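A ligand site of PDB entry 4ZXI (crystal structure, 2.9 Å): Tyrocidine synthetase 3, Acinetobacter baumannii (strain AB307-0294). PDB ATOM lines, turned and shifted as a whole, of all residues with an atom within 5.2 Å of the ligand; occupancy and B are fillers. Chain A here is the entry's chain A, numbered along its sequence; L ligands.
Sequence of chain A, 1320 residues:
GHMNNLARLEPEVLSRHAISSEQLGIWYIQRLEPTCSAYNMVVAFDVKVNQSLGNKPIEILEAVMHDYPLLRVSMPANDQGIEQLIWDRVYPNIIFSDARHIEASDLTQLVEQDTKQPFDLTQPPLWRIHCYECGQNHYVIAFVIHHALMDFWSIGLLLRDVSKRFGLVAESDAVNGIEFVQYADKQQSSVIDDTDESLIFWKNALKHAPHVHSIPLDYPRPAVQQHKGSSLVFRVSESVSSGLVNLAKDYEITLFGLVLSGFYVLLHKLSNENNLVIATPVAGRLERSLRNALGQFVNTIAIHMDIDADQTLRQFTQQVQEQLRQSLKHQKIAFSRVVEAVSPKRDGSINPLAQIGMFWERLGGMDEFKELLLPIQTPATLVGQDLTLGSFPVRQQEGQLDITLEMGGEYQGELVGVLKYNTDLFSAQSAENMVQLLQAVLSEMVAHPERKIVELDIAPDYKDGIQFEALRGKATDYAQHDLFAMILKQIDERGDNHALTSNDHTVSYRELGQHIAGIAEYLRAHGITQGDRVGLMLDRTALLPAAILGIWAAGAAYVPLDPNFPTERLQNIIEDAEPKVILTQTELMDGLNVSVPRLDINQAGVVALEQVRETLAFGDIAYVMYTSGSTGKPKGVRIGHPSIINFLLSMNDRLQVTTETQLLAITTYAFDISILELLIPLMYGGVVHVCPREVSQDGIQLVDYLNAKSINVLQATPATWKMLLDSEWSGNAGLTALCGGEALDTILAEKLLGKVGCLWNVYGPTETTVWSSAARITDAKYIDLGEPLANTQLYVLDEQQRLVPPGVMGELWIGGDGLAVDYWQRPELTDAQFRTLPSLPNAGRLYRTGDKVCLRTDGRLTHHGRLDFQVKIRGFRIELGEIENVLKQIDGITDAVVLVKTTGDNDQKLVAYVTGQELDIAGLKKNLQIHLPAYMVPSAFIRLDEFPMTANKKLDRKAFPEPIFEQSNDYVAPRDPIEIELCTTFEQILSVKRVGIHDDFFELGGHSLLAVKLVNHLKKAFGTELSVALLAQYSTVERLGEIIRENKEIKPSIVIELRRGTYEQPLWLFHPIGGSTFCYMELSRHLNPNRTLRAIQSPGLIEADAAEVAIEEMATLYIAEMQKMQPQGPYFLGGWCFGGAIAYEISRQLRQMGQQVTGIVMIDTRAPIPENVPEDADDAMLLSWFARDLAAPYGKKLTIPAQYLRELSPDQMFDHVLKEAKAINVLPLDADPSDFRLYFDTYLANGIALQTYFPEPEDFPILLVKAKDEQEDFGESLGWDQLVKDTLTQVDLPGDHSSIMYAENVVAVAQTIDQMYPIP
Gly 25 touches the ligand. CD1 of Ile 29 touches N1 of the ligand, 3.6 Å away. CE2 of Phe 335 touches C7 of the ligand, at 3.7 Å. CB of Ser 336 touches C3 of the ligand (3.6 Å). Val 339 touches the ligand. Pro 352 touches the ligand (CD to O4, 3.7 Å). His 1007 touches the ligand (C to O2, 3.7 Å). Hydrophobic or aromatic side chains within 4 Å of the ligand: Ile 29, Tyr 39, Phe 335, Val 339, Pro 352 and His 1007. Within 4 Å of the ligand: Gly 25, Ile 29, Tyr 39, His 147, Thr 300, Phe 335, Ser 336, Val 339, Arg 346, Asn 351, Pro 352, His 1007 and Ser 1008.
The backbone NH (N) of His 147 is in hydrogen-bond range of the backbone carbonyl oxygen (O) of Tyr 39 (2.8 Å).
An oxygen (O2) of the ligand sits at hydrogen-bond distance from the backbone NH (N) of Ser 1008. A phosphorus (P1) of the ligand is bonded to the side-chain hydroxyl of Ser 1008 (1.6 Å). The side-chain hydroxyl of Tyr 39 lies within hydrogen-bond range of a nitrogen (N2) of the ligand (2.9 Å). NE of Arg 346 sits at hydrogen-bond distance from O1 of the ligand. N1 of the ligand lies within hydrogen-bond range of OD1 of Asn 351 (3.0 Å). The side-chain hydroxyl (OG1) of Thr 300 is in hydrogen-bond range of an oxygen (O6) of the ligand, at 3.4 Å. A sulfur (S1) of the ligand lies close to a ring nitrogen (NE2) of His 147, at 3.7 Å.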
ATOM      1  N   GLY A  25      26.684 -15.467   0.177  1.00  0.00           N
ATOM      2  CA  GLY A  25      26.641 -14.636  -1.014  1.00  0.00           C
ATOM      3  C   GLY A  25      25.266 -14.549  -1.638  1.00  0.00           C
ATOM      4  O   GLY A  25      24.762 -13.463  -1.928  1.00  0.00           O
ATOM      5  N   ILE A  26      24.648 -15.705  -1.852  1.00  0.00           N
ATOM      6  CA  ILE A  26      23.310 -15.749  -2.411  1.00  0.00           C
ATOM      7  C   ILE A  26      22.339 -15.027  -1.480  1.00  0.00           C
ATOM      8  O   ILE A  26      21.514 -14.237  -1.933  1.00  0.00           O
ATOM      9  CB  ILE A  26      22.884 -17.215  -2.668  1.00  0.00           C
ATOM     10  CG1 ILE A  26      23.733 -17.772  -3.808  1.00  0.00           C
ATOM     11  CG2 ILE A  26      21.405 -17.323  -2.957  1.00  0.00           C
ATOM     12  CD1 ILE A  26      23.591 -19.242  -4.068  1.00  0.00           C
ATOM     13  N   TYR A  28      22.940 -12.609   0.614  1.00  0.00           N
ATOM     14  CA  TYR A  28      23.195 -11.181   0.560  1.00  0.00           C
ATOM     15  C   TYR A  28      22.576 -10.581  -0.687  1.00  0.00           C
ATOM     16  O   TYR A  28      21.986  -9.505  -0.632  1.00  0.00           O
ATOM     17  CB  TYR A  28      24.684 -10.912   0.597  1.00  0.00           C
ATOM     18  CG  TYR A  28      25.080  -9.477   0.450  1.00  0.00           C
ATOM     19  CD1 TYR A  28      25.160  -8.632   1.547  1.00  0.00           C
ATOM     20  CD2 TYR A  28      25.403  -8.955  -0.804  1.00  0.00           C
ATOM     21  CE1 TYR A  28      25.560  -7.295   1.399  1.00  0.00           C
ATOM     22  CE2 TYR A  28      25.783  -7.632  -0.956  1.00  0.00           C
ATOM     23  CZ  TYR A  28      25.859  -6.817   0.150  1.00  0.00           C
ATOM     24  OH  TYR A  28      26.241  -5.505  -0.030  1.00  0.00           O
ATOM     25  N   ILE A  29      22.690 -11.282  -1.807  1.00  0.00           N
ATOM     26  CA  ILE A  29      22.128 -10.776  -3.051  1.00  0.00           C
ATOM     27  C   ILE A  29      20.609 -10.679  -2.925  1.00  0.00           C
ATOM     28  O   ILE A  29      20.007  -9.671  -3.341  1.00  0.00           O
ATOM     29  CB  ILE A  29      22.516 -11.658  -4.232  1.00  0.00           C
ATOM     30  CG1 ILE A  29      24.036 -11.616  -4.408  1.00  0.00           C
ATOM     31  CG2 ILE A  29      21.794 -11.232  -5.507  1.00  0.00           C
ATOM     32  CD1 ILE A  29      24.559 -12.570  -5.426  1.00  0.00           C
ATOM     33  N   TYR A  39      17.524 -16.817  -8.212  1.00  0.00           N
ATOM     34  CA  TYR A  39      17.961 -17.997  -7.489  1.00  0.00           C
ATOM     35  C   TYR A  39      16.766 -18.860  -7.069  1.00  0.00           C
ATOM     36  O   TYR A  39      16.851 -19.666  -6.146  1.00  0.00           O
ATOM     37  CB  TYR A  39      18.827 -17.580  -6.292  1.00  0.00           C
ATOM     38  CG  TYR A  39      20.118 -16.963  -6.744  1.00  0.00           C
ATOM     39  CD1 TYR A  39      21.230 -17.741  -7.026  1.00  0.00           C
ATOM     40  CD2 TYR A  39      20.218 -15.593  -6.945  1.00  0.00           C
ATOM     41  CE1 TYR A  39      22.412 -17.181  -7.462  1.00  0.00           C
ATOM     42  CE2 TYR A  39      21.403 -15.024  -7.382  1.00  0.00           C
ATOM     43  CZ  TYR A  39      22.498 -15.817  -7.645  1.00  0.00           C
ATOM     44  OH  TYR A  39      23.672 -15.265  -8.090  1.00  0.00           O
ATOM     45  N   HIS A 147      17.825 -20.939  -3.808  1.00  0.00           N
ATOM     46  CA  HIS A 147      19.164 -21.526  -3.883  1.00  0.00           C
ATOM     47  C   HIS A 147      19.968 -21.301  -2.588  1.00  0.00           C
ATOM     48  O   HIS A 147      20.962 -21.976  -2.349  1.00  0.00           O
ATOM     49  CB  HIS A 147      19.910 -20.952  -5.090  1.00  0.00           C
ATOM     50  CG  HIS A 147      20.957 -21.858  -5.647  1.00  0.00           C
ATOM     51  ND1 HIS A 147      21.843 -22.552  -4.852  1.00  0.00           N
ATOM     52  CD2 HIS A 147      21.306 -22.140  -6.926  1.00  0.00           C
ATOM     53  CE1 HIS A 147      22.674 -23.250  -5.612  1.00  0.00           C
ATOM     54  NE2 HIS A 147      22.371 -23.004  -6.880  1.00  0.00           N
ATOM     55  N   PRO A 281      30.468 -22.833 -11.181  1.00  0.00           N
ATOM     56  CA  PRO A 281      30.064 -23.611 -10.011  1.00  0.00           C
ATOM     57  C   PRO A 281      30.896 -24.875  -9.814  1.00  0.00           C
ATOM     58  O   PRO A 281      31.316 -25.528 -10.783  1.00  0.00           O
ATOM     59  CB  PRO A 281      28.627 -23.987 -10.329  1.00  0.00           C
ATOM     60  CG  PRO A 281      28.165 -22.942 -11.245  1.00  0.00           C
ATOM     61  CD  PRO A 281      29.341 -22.613 -12.099  1.00  0.00           C
ATOM     62  N   VAL A 298      27.284 -25.472  -3.001  1.00  0.00           N
ATOM     63  CA  VAL A 298      27.918 -25.102  -4.236  1.00  0.00           C
ATOM     64  C   VAL A 298      28.744 -23.850  -4.040  1.00  0.00           C
ATOM     65  O   VAL A 298      28.263 -22.845  -3.509  1.00  0.00           O
ATOM     66  CB  VAL A 298      26.886 -24.879  -5.351  1.00  0.00           C
ATOM     67  CG1 VAL A 298      27.541 -24.283  -6.594  1.00  0.00           C
ATOM     68  CG2 VAL A 298      26.298 -26.158  -5.718  1.00  0.00           C
ATOM     69  N   THR A 300      31.273 -20.967  -6.056  1.00  0.00           N
ATOM     70  CA  THR A 300      31.644 -20.407  -7.352  1.00  0.00           C
ATOM     71  C   THR A 300      33.145 -20.108  -7.387  1.00  0.00           C
ATOM     72  O   THR A 300      33.682 -19.580  -6.419  1.00  0.00           O
ATOM     73  CB  THR A 300      30.869 -19.140  -7.653  1.00  0.00           C
ATOM     74  OG1 THR A 300      29.465 -19.430  -7.627  1.00  0.00           O
ATOM     75  CG2 THR A 300      31.235 -18.587  -9.007  1.00  0.00           C
ATOM     76  N   PHE A 335      33.586 -17.910  -2.787  1.00  0.00           N
ATOM     77  CA  PHE A 335      33.689 -16.746  -3.665  1.00  0.00           C
ATOM     78  C   PHE A 335      33.509 -15.429  -2.896  1.00  0.00           C
ATOM     79  O   PHE A 335      34.231 -14.468  -3.157  1.00  0.00           O
ATOM     80  CB  PHE A 335      32.665 -16.833  -4.798  1.00  0.00           C
ATOM     81  CG  PHE A 335      32.738 -15.700  -5.762  1.00  0.00           C
ATOM     82  CD1 PHE A 335      33.757 -15.653  -6.708  1.00  0.00           C
ATOM     83  CD2 PHE A 335      31.794 -14.689  -5.738  1.00  0.00           C
ATOM     84  CE1 PHE A 335      33.831 -14.606  -7.608  1.00  0.00           C
ATOM     85  CE2 PHE A 335      31.855 -13.637  -6.642  1.00  0.00           C
ATOM     86  CZ  PHE A 335      32.879 -13.593  -7.579  1.00  0.00           C
ATOM     87  N   SER A 336      32.588 -15.405  -1.932  1.00  0.00           N
ATOM     88  CA  SER A 336      32.421 -14.244  -1.065  1.00  0.00           C
ATOM     89  C   SER A 336      33.733 -13.907  -0.374  1.00  0.00           C
ATOM     90  O   SER A 336      34.088 -12.732  -0.227  1.00  0.00           O
ATOM     91  CB  SER A 336      31.344 -14.474  -0.021  1.00  0.00           C
ATOM     92  OG  SER A 336      31.851 -15.316   1.011  1.00  0.00           O
ATOM     93  N   VAL A 339      36.161 -12.354  -2.938  1.00  0.00           N
ATOM     94  CA  VAL A 339      35.814 -10.973  -3.216  1.00  0.00           C
ATOM     95  C   VAL A 339      36.306 -10.094  -2.081  1.00  0.00           C
ATOM     96  O   VAL A 339      36.813  -8.993  -2.324  1.00  0.00           O
ATOM     97  CB  VAL A 339      34.312 -10.767  -3.418  1.00  0.00           C
ATOM     98  CG1 VAL A 339      33.993  -9.273  -3.544  1.00  0.00           C
ATOM     99  CG2 VAL A 339      33.886 -11.476  -4.671  1.00  0.00           C
ATOM    100  N   ARG A 346      33.501  -1.817  -5.480  1.00  0.00           N
ATOM    101  CA  ARG A 346      32.099  -2.265  -5.503  1.00  0.00           C
ATOM    102  C   ARG A 346      31.352  -1.373  -6.488  1.00  0.00           C
ATOM    103  O   ARG A 346      31.647  -0.190  -6.623  1.00  0.00           O
ATOM    104  CB  ARG A 346      31.424  -2.232  -4.138  1.00  0.00           C
ATOM    105  CG  ARG A 346      32.061  -3.130  -3.089  1.00  0.00           C
ATOM    106  CD  ARG A 346      32.412  -4.524  -3.621  1.00  0.00           C
ATOM    107  NE  ARG A 346      32.742  -5.422  -2.510  1.00  0.00           N
ATOM    108  CZ  ARG A 346      33.941  -5.467  -1.925  1.00  0.00           C
ATOM    109  NH1 ARG A 346      34.919  -4.677  -2.354  1.00  0.00           N
ATOM    110  NH2 ARG A 346      34.171  -6.305  -0.918  1.00  0.00           N
ATOM    111  N   ASN A 351      28.070  -7.873 -11.068  1.00  0.00           N
ATOM    112  CA  ASN A 351      28.585  -8.812 -10.087  1.00  0.00           C
ATOM    113  C   ASN A 351      30.098  -8.649  -9.923  1.00  0.00           C
ATOM    114  O   ASN A 351      30.816  -8.484 -10.913  1.00  0.00           O
ATOM    115  CB  ASN A 351      28.251 -10.221 -10.515  1.00  0.00           C
ATOM    116  CG  ASN A 351      28.544 -11.210  -9.450  1.00  0.00           C
ATOM    117  OD1 ASN A 351      27.802 -11.292  -8.463  1.00  0.00           O
ATOM    118  ND2 ASN A 351      29.627 -11.970  -9.616  1.00  0.00           N
ATOM    119  N   PRO A 352      30.599  -8.677  -8.674  1.00  0.00           N
ATOM    120  CA  PRO A 352      32.051  -8.526  -8.465  1.00  0.00           C
ATOM    121  C   PRO A 352      32.883  -9.564  -9.222  1.00  0.00           C
ATOM    122  O   PRO A 352      32.428 -10.682  -9.416  1.00  0.00           O
ATOM    123  CB  PRO A 352      32.208  -8.705  -6.965  1.00  0.00           C
ATOM    124  CG  PRO A 352      30.851  -8.432  -6.385  1.00  0.00           C
ATOM    125  CD  PRO A 352      29.841  -8.824  -7.420  1.00  0.00           C
ATOM    126  N   PHE A 359      27.959 -22.969 -16.507  1.00  0.00           N
ATOM    127  CA  PHE A 359      27.581 -24.108 -15.662  1.00  0.00           C
ATOM    128  C   PHE A 359      27.705 -25.361 -16.490  1.00  0.00           C
ATOM    129  O   PHE A 359      27.197 -25.419 -17.613  1.00  0.00           O
ATOM    130  CB  PHE A 359      26.134 -23.994 -15.136  1.00  0.00           C
ATOM    131  CG  PHE A 359      25.874 -22.821 -14.247  1.00  0.00           C
ATOM    132  CD1 PHE A 359      26.768 -21.749 -14.157  1.00  0.00           C
ATOM    133  CD2 PHE A 359      24.731 -22.788 -13.470  1.00  0.00           C
ATOM    134  CE1 PHE A 359      26.512 -20.651 -13.335  1.00  0.00           C
ATOM    135  CE2 PHE A 359      24.469 -21.699 -12.634  1.00  0.00           C
ATOM    136  CZ  PHE A 359      25.369 -20.628 -12.572  1.00  0.00           C
ATOM    137  N   GLN A 400      21.110 -14.117 -13.132  1.00  0.00           N
ATOM    138  CA  GLN A 400      22.245 -14.180 -12.206  1.00  0.00           C
ATOM    139  C   GLN A 400      23.447 -13.341 -12.660  1.00  0.00           C
ATOM    140  O   GLN A 400      23.975 -12.550 -11.875  1.00  0.00           O
ATOM    141  CB  GLN A 400      22.700 -15.618 -12.017  1.00  0.00           C
ATOM    142  CG  GLN A 400      21.909 -16.383 -11.006  1.00  0.00           C
ATOM    143  CD  GLN A 400      22.232 -17.863 -11.069  1.00  0.00           C
ATOM    144  OE1 GLN A 400      23.117 -18.283 -11.832  1.00  0.00           O
ATOM    145  NE2 GLN A 400      21.523 -18.673 -10.283  1.00  0.00           N
ATOM    146  N   LEU A 401      23.877 -13.524 -13.905  1.00  0.00           N
ATOM    147  CA  LEU A 401      25.006 -12.763 -14.429  1.00  0.00           C
ATOM    148  C   LEU A 401      24.632 -12.068 -15.728  1.00  0.00           C
ATOM    149  O   LEU A 401      23.459 -12.027 -16.103  1.00  0.00           O
ATOM    150  CB  LEU A 401      26.219 -13.674 -14.623  1.00  0.00           C
ATOM    151  CG  LEU A 401      26.663 -14.446 -13.384  1.00  0.00           C
ATOM    152  CD1 LEU A 401      27.673 -15.460 -13.755  1.00  0.00           C
ATOM    153  CD2 LEU A 401      27.274 -13.520 -12.356  1.00  0.00           C
ATOM    154  N   HIS A1007      33.216  -4.871   3.451  1.00  0.00           N
ATOM    155  CA  HIS A1007      32.807  -5.901   2.516  1.00  0.00           C
ATOM    156  C   HIS A1007      31.399  -6.358   2.862  1.00  0.00           C
ATOM    157  O   HIS A1007      30.850  -5.957   3.895  1.00  0.00           O
ATOM    158  CB  HIS A1007      33.784  -7.063   2.544  1.00  0.00           C
ATOM    159  CG  HIS A1007      33.980  -7.634   3.907  1.00  0.00           C
ATOM    160  ND1 HIS A1007      33.095  -8.524   4.469  1.00  0.00           N
ATOM    161  CD2 HIS A1007      34.939  -7.412   4.837  1.00  0.00           C
ATOM    162  CE1 HIS A1007      33.503  -8.837   5.684  1.00  0.00           C
ATOM    163  NE2 HIS A1007      34.627  -8.179   5.932  1.00  0.00           N
ATOM    164  N   SER A1008      30.827  -7.217   2.027  1.00  0.00           N
ATOM    165  CA  SER A1008      29.381  -7.428   2.026  1.00  0.00           C
ATOM    166  C   SER A1008      28.806  -7.917   3.353  1.00  0.00           C
ATOM    167  O   SER A1008      27.825  -7.339   3.818  1.00  0.00           O
ATOM    168  CB  SER A1008      28.985  -8.395   0.909  1.00  0.00           C
ATOM    169  OG  SER A1008      29.044  -7.695  -0.325  1.00  0.00           O
ATOM    170  N   LEU A1009      29.393  -8.945   3.962  1.00  0.00           N
ATOM    171  CA  LEU A1009      28.902  -9.389   5.262  1.00  0.00           C
ATOM    172  C   LEU A1009      28.958  -8.258   6.310  1.00  0.00           C
ATOM    173  O   LEU A1009      28.035  -8.133   7.109  1.00  0.00           O
ATOM    174  CB  LEU A1009      29.683 -10.610   5.736  1.00  0.00           C
ATOM    175  CG  LEU A1009      29.484 -11.201   7.136  1.00  0.00           C
ATOM    176  CD1 LEU A1009      28.046 -11.151   7.594  1.00  0.00           C
ATOM    177  CD2 LEU A1009      29.954 -12.639   7.104  1.00  0.00           C
HETATM  178  O1  LIG L   1      30.270  -7.001  -2.462  1.00  0.00           O
HETATM  179  P1  LIG L   1      30.356  -7.953  -1.278  1.00  0.00           P
HETATM  180  O2  LIG L   1      31.623  -7.943  -0.472  1.00  0.00           O
HETATM  181  O3  LIG L   1      30.170  -9.475  -1.820  1.00  0.00           O
HETATM  182  C1  LIG L   1      29.000  -9.871  -2.548  1.00  0.00           C
HETATM  183  C2  LIG L   1      29.192 -11.272  -3.108  1.00  0.00           C
HETATM  184  C3  LIG L   1      29.251 -12.162  -1.882  1.00  0.00           C
HETATM  185  C4  LIG L   1      30.490 -11.317  -3.908  1.00  0.00           C
HETATM  186  C5  LIG L   1      28.004 -11.657  -4.000  1.00  0.00           C
HETATM  187  O4  LIG L   1      27.721 -10.590  -4.922  1.00  0.00           O
HETATM  188  C6  LIG L   1      28.167 -13.001  -4.707  1.00  0.00           C
HETATM  189  O5  LIG L   1      28.302 -14.051  -4.072  1.00  0.00           O
HETATM  190  N1  LIG L   1      28.073 -13.051  -6.037  1.00  0.00           N
HETATM  191  C7  LIG L   1      28.183 -14.268  -6.848  1.00  0.00           C
HETATM  192  C8  LIG L   1      26.829 -15.010  -6.839  1.00  0.00           C
HETATM  193  C9  LIG L   1      26.968 -16.235  -7.716  1.00  0.00           C
HETATM  194  O6  LIG L   1      28.027 -16.467  -8.277  1.00  0.00           O
HETATM  195  N2  LIG L   1      25.950 -17.081  -7.881  1.00  0.00           N
HETATM  196  C10 LIG L   1      26.003 -18.288  -8.727  1.00  0.00           C
HETATM  197  C11 LIG L   1      25.889 -19.512  -7.797  1.00  0.00           C
HETATM  198  S1  LIG L   1      24.910 -20.877  -8.521  1.00  0.00           S
